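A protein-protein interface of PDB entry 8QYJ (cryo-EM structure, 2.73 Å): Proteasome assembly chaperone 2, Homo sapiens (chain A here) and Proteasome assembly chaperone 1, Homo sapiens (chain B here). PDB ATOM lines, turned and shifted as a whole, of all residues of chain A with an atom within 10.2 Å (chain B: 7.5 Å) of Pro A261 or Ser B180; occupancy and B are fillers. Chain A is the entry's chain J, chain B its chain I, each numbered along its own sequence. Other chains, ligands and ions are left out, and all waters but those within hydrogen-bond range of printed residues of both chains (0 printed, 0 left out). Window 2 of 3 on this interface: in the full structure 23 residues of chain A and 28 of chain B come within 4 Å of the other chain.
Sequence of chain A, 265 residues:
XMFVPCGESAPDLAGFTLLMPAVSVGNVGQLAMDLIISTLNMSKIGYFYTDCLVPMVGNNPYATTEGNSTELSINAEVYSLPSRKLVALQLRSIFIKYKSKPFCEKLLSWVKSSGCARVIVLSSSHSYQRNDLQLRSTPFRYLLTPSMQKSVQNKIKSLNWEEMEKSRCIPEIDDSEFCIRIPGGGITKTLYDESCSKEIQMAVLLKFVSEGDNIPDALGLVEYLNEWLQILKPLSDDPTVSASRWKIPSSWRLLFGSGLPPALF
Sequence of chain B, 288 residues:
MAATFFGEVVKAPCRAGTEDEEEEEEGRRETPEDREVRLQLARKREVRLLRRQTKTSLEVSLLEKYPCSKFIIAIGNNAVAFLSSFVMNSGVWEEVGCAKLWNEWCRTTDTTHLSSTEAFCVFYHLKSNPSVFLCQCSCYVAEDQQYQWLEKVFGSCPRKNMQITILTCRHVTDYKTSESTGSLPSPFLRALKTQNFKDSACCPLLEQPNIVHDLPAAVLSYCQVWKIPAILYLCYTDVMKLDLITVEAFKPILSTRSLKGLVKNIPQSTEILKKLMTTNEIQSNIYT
O of Tyr B175 sits at hydrogen-bond distance from OG of Ser A258. N of Gly A259 is in hydrogen-bond range of O of Glu B179, 3.0 Å away.
OG1 of Thr B177 lies close to OE2 of Glu B179. The side-chain hydroxyl (OG) of Ser B178 sits at hydrogen-bond distance from the side-chain carboxylate (OE1) of Glu B179 (3.1 Å). OG of Ser B183 sits at hydrogen-bond distance from O of Ser B180 (3.1 Å).
Leu A254 touches Thr B177 (CD2 to O, 3.8 Å). Ser A258 touches Thr B177 (CA to O, 3.3 Å). Glu B179 touches Ser A258. Ser A258 touches Thr B181 (OG to OG1, 3.8 Å). Gly A259 touches Thr B177 (N to O, 3.6 Å). Ser B178 touches Gly A259 (O to CA, 3.4 Å). Pro A261 touches Ser B180.
Pro A261 touches one residue of chain B. Ser B180 touches just one residue of chain A: Pro A261. Of chain A, only Ser A258 (3.96 Å) and Gly A259 (3.0 Å) come within 4 Å of Glu B179. Of chain A, only Ser A258 comes within 4 Å of Thr B181. No residue of chain A comes within 4 Å of Gly B182. No residue of chain A comes within 4 Å of Ser B183. Of the printed residues of chain B, Leu A254 touches Thr B177 (3.8 Å). Printed residues of chain A within 4 Å of Tyr B175: Ser A258. Of the printed residues of chain B, Ser A258 touches Tyr B175 (3.4 Å), Thr B177 (3.3 Å), Glu B179 (3.96 Å) and Thr B181 (3.8 Å). Printed residues of chain A within 4 Å of Thr B177: Leu A254 (3.8 Å), Ser A258 (3.3 Å) and Gly A259 (3.6 Å). Leu A264 touches none of the printed residues of chain B. Phe A265 touches none of the printed residues of chain B. The nearest residue of chain A that does not touch Ser B180 is Leu A260 (4.1 Å). The nearest printed residue of chain A that does not touch Tyr B175 is Gly A257 (6.6 Å).
Of the 10 printed residues of chain A, 4 touch a printed residue of chain B. Of the 9 printed residues of chain B, 6 touch a printed residue of chain A. Along chain B the printed residues that touch a printed residue of chain A span positions 175 to 181. Among the printed residues, 9 pairs touch across the chains. Among the printed residues, no Asp or Glu carboxylate lies within 4 Å of a Lys or Arg side-chain nitrogen of the other chain.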
ATOM      1  N   LEU A 254     -17.865   6.844  13.258  1.00  0.00           N
ATOM      2  CA  LEU A 254     -18.356   5.761  14.105  1.00  0.00           C
ATOM      3  C   LEU A 254     -19.103   4.733  13.270  1.00  0.00           C
ATOM      4  O   LEU A 254     -20.233   4.345  13.572  1.00  0.00           O
ATOM      5  CB  LEU A 254     -19.241   6.306  15.222  1.00  0.00           C
ATOM      6  CG  LEU A 254     -18.562   7.234  16.232  1.00  0.00           C
ATOM      7  CD1 LEU A 254     -19.528   8.299  16.718  1.00  0.00           C
ATOM      8  CD2 LEU A 254     -18.002   6.443  17.399  1.00  0.00           C
ATOM      9  N   GLY A 257     -20.520   1.852  15.271  1.00  0.00           N
ATOM     10  CA  GLY A 257     -21.419   2.085  16.385  1.00  0.00           C
ATOM     11  C   GLY A 257     -20.825   2.915  17.505  1.00  0.00           C
ATOM     12  O   GLY A 257     -19.923   3.725  17.279  1.00  0.00           O
ATOM     13  N   SER A 258     -21.328   2.719  18.722  1.00  0.00           N
ATOM     14  CA  SER A 258     -20.878   3.467  19.885  1.00  0.00           C
ATOM     15  C   SER A 258     -19.744   2.714  20.582  1.00  0.00           C
ATOM     16  O   SER A 258     -19.183   1.754  20.048  1.00  0.00           O
ATOM     17  CB  SER A 258     -22.050   3.731  20.827  1.00  0.00           C
ATOM     18  OG  SER A 258     -23.080   4.444  20.170  1.00  0.00           O
ATOM     19  N   GLY A 259     -19.396   3.147  21.793  1.00  0.00           N
ATOM     20  CA  GLY A 259     -18.284   2.577  22.519  1.00  0.00           C
ATOM     21  C   GLY A 259     -18.612   1.254  23.185  1.00  0.00           C
ATOM     22  O   GLY A 259     -19.747   0.777  23.191  1.00  0.00           O
ATOM     23  N   LEU A 260     -17.576   0.656  23.764  1.00  0.00           N
ATOM     24  CA  LEU A 260     -17.688  -0.655  24.393  1.00  0.00           C
ATOM     25  C   LEU A 260     -18.196  -0.515  25.825  1.00  0.00           C
ATOM     26  O   LEU A 260     -17.686   0.322  26.577  1.00  0.00           O
ATOM     27  CB  LEU A 260     -16.335  -1.361  24.384  1.00  0.00           C
ATOM     28  CG  LEU A 260     -16.250  -2.763  24.987  1.00  0.00           C
ATOM     29  CD1 LEU A 260     -16.897  -3.787  24.073  1.00  0.00           C
ATOM     30  CD2 LEU A 260     -14.802  -3.128  25.264  1.00  0.00           C
ATOM     31  N   PRO A 261     -19.194  -1.303  26.232  1.00  0.00           N
ATOM     32  CA  PRO A 261     -19.671  -1.216  27.612  1.00  0.00           C
ATOM     33  C   PRO A 261     -18.623  -1.730  28.580  1.00  0.00           C
ATOM     34  O   PRO A 261     -17.798  -2.592  28.227  1.00  0.00           O
ATOM     35  CB  PRO A 261     -20.924  -2.113  27.612  1.00  0.00           C
ATOM     36  CG  PRO A 261     -21.240  -2.371  26.171  1.00  0.00           C
ATOM     37  CD  PRO A 261     -19.942  -2.296  25.448  1.00  0.00           C
ATOM     38  N   PRO A 262     -18.615  -1.237  29.813  1.00  0.00           N
ATOM     39  CA  PRO A 262     -17.629  -1.695  30.796  1.00  0.00           C
ATOM     40  C   PRO A 262     -18.039  -3.019  31.429  1.00  0.00           C
ATOM     41  O   PRO A 262     -19.122  -3.554  31.186  1.00  0.00           O
ATOM     42  CB  PRO A 262     -17.608  -0.568  31.841  1.00  0.00           C
ATOM     43  CG  PRO A 262     -18.499   0.527  31.294  1.00  0.00           C
ATOM     44  CD  PRO A 262     -19.429  -0.129  30.332  1.00  0.00           C
ATOM     45  N   ALA A 263     -17.129  -3.543  32.254  1.00  0.00           N
ATOM     46  CA  ALA A 263     -17.351  -4.766  33.030  1.00  0.00           C
ATOM     47  C   ALA A 263     -17.598  -5.977  32.132  1.00  0.00           C
ATOM     48  O   ALA A 263     -18.383  -6.867  32.462  1.00  0.00           O
ATOM     49  CB  ALA A 263     -18.498  -4.588  34.027  1.00  0.00           C
ATOM     50  N   LEU A 264     -16.922  -6.013  30.985  1.00  0.00           N
ATOM     51  CA  LEU A 264     -16.927  -7.182  30.114  1.00  0.00           C
ATOM     52  C   LEU A 264     -15.537  -7.760  29.910  1.00  0.00           C
ATOM     53  O   LEU A 264     -15.353  -8.977  30.021  1.00  0.00           O
ATOM     54  CB  LEU A 264     -17.550  -6.837  28.751  1.00  0.00           C
ATOM     55  CG  LEU A 264     -19.047  -6.542  28.719  1.00  0.00           C
ATOM     56  CD1 LEU A 264     -19.468  -6.099  27.330  1.00  0.00           C
ATOM     57  CD2 LEU A 264     -19.830  -7.768  29.148  1.00  0.00           C
ATOM     58  N   PHE A 265     -14.552  -6.920  29.613  1.00  0.00           N
ATOM     59  CA  PHE A 265     -13.195  -7.384  29.357  1.00  0.00           C
ATOM     60  C   PHE A 265     -12.255  -6.964  30.481  1.00  0.00           C
ATOM     61  O   PHE A 265     -11.365  -7.718  30.874  1.00  0.00           O
ATOM     62  CB  PHE A 265     -12.691  -6.843  28.018  1.00  0.00           C
ATOM     63  CG  PHE A 265     -13.469  -7.338  26.834  1.00  0.00           C
ATOM     64  CD1 PHE A 265     -13.102  -8.504  26.185  1.00  0.00           C
ATOM     65  CD2 PHE A 265     -14.568  -6.638  26.369  1.00  0.00           C
ATOM     66  CE1 PHE A 265     -13.816  -8.961  25.096  1.00  0.00           C
ATOM     67  CE2 PHE A 265     -15.285  -7.091  25.280  1.00  0.00           C
ATOM     68  CZ  PHE A 265     -14.908  -8.253  24.643  1.00  0.00           C
ATOM     69  N   TYR B 175     -28.557   7.165  19.784  1.00  0.00           N
ATOM     70  CA  TYR B 175     -27.494   8.159  19.777  1.00  0.00           C
ATOM     71  C   TYR B 175     -26.142   7.495  19.553  1.00  0.00           C
ATOM     72  O   TYR B 175     -25.884   6.396  20.050  1.00  0.00           O
ATOM     73  CB  TYR B 175     -27.491   8.930  21.096  1.00  0.00           C
ATOM     74  CG  TYR B 175     -26.783  10.261  21.038  1.00  0.00           C
ATOM     75  CD1 TYR B 175     -27.342  11.337  20.366  1.00  0.00           C
ATOM     76  CD2 TYR B 175     -25.561  10.445  21.667  1.00  0.00           C
ATOM     77  CE1 TYR B 175     -26.700  12.556  20.315  1.00  0.00           C
ATOM     78  CE2 TYR B 175     -24.912  11.659  21.622  1.00  0.00           C
ATOM     79  CZ  TYR B 175     -25.485  12.712  20.944  1.00  0.00           C
ATOM     80  OH  TYR B 175     -24.840  13.924  20.897  1.00  0.00           O
ATOM     81  N   THR B 177     -22.050   7.906  19.978  1.00  0.00           N
ATOM     82  CA  THR B 177     -21.028   8.618  20.730  1.00  0.00           C
ATOM     83  C   THR B 177     -19.800   7.729  20.855  1.00  0.00           C
ATOM     84  O   THR B 177     -19.877   6.507  20.711  1.00  0.00           O
ATOM     85  CB  THR B 177     -21.537   9.039  22.115  1.00  0.00           C
ATOM     86  OG1 THR B 177     -20.487   9.696  22.835  1.00  0.00           O
ATOM     87  CG2 THR B 177     -22.008   7.828  22.902  1.00  0.00           C
ATOM     88  N   SER B 178     -18.656   8.364  21.123  1.00  0.00           N
ATOM     89  CA  SER B 178     -17.409   7.616  21.238  1.00  0.00           C
ATOM     90  C   SER B 178     -17.388   6.734  22.481  1.00  0.00           C
ATOM     91  O   SER B 178     -16.795   5.650  22.456  1.00  0.00           O
ATOM     92  CB  SER B 178     -16.220   8.576  21.248  1.00  0.00           C
ATOM     93  OG  SER B 178     -16.441   9.654  22.140  1.00  0.00           O
ATOM     94  N   GLU B 179     -18.017   7.174  23.566  1.00  0.00           N
ATOM     95  CA  GLU B 179     -18.062   6.401  24.797  1.00  0.00           C
ATOM     96  C   GLU B 179     -19.304   5.511  24.802  1.00  0.00           C
ATOM     97  O   GLU B 179     -19.995   5.360  23.791  1.00  0.00           O
ATOM     98  CB  GLU B 179     -18.017   7.331  26.007  1.00  0.00           C
ATOM     99  CG  GLU B 179     -19.144   8.343  26.060  1.00  0.00           C
ATOM    100  CD  GLU B 179     -18.718   9.708  25.560  1.00  0.00           C
ATOM    101  OE1 GLU B 179     -17.634   9.805  24.948  1.00  0.00           O
ATOM    102  OE2 GLU B 179     -19.464  10.684  25.782  1.00  0.00           O
ATOM    103  N   SER B 180     -19.596   4.901  25.948  1.00  0.00           N
ATOM    104  CA  SER B 180     -20.734   4.000  26.050  1.00  0.00           C
ATOM    105  C   SER B 180     -22.046   4.778  26.091  1.00  0.00           C
ATOM    106  O   SER B 180     -22.100   5.931  26.526  1.00  0.00           O
ATOM    107  CB  SER B 180     -20.609   3.123  27.294  1.00  0.00           C
ATOM    108  OG  SER B 180     -21.549   2.064  27.263  1.00  0.00           O
ATOM    109  N   THR B 181     -23.113   4.124  25.628  1.00  0.00           N
ATOM    110  CA  THR B 181     -24.430   4.753  25.628  1.00  0.00           C
ATOM    111  C   THR B 181     -24.961   4.929  27.046  1.00  0.00           C
ATOM    112  O   THR B 181     -25.588   5.949  27.360  1.00  0.00           O
ATOM    113  CB  THR B 181     -25.403   3.924  24.785  1.00  0.00           C
ATOM    114  OG1 THR B 181     -25.010   3.977  23.408  1.00  0.00           O
ATOM    115  CG2 THR B 181     -26.822   4.455  24.915  1.00  0.00           C
ATOM    116  N   GLY B 182     -24.704   3.959  27.923  1.00  0.00           N
ATOM    117  CA  GLY B 182     -25.264   3.987  29.263  1.00  0.00           C
ATOM    118  C   GLY B 182     -24.620   4.984  30.203  1.00  0.00           C
ATOM    119  O   GLY B 182     -25.127   5.170  31.315  1.00  0.00           O
ATOM    120  N   SER B 183     -23.527   5.620  29.794  1.00  0.00           N
ATOM    121  CA  SER B 183     -22.856   6.614  30.620  1.00  0.00           C
ATOM    122  C   SER B 183     -23.366   8.029  30.384  1.00  0.00           C
ATOM    123  O   SER B 183     -22.918   8.955  31.069  1.00  0.00           O
ATOM    124  CB  SER B 183     -21.344   6.565  30.376  1.00  0.00           C
ATOM    125  OG  SER B 183     -21.010   7.149  29.130  1.00  0.00           O
ATOM    126  N   LEU B 184     -24.283   8.221  29.438  1.00  0.00           N
ATOM    127  CA  LEU B 184     -24.797   9.546  29.135  1.00  0.00           C
ATOM    128  C   LEU B 184     -25.831   9.979  30.173  1.00  0.00           C
ATOM    129  O   LEU B 184     -26.554   9.147  30.727  1.00  0.00           O
ATOM    130  CB  LEU B 184     -25.426   9.564  27.746  1.00  0.00           C
ATOM    131  CG  LEU B 184     -24.474   9.347  26.569  1.00  0.00           C
ATOM    132  CD1 LEU B 184     -25.253   9.074  25.295  1.00  0.00           C
ATOM    133  CD2 LEU B 184     -23.558  10.543  26.392  1.00  0.00           C
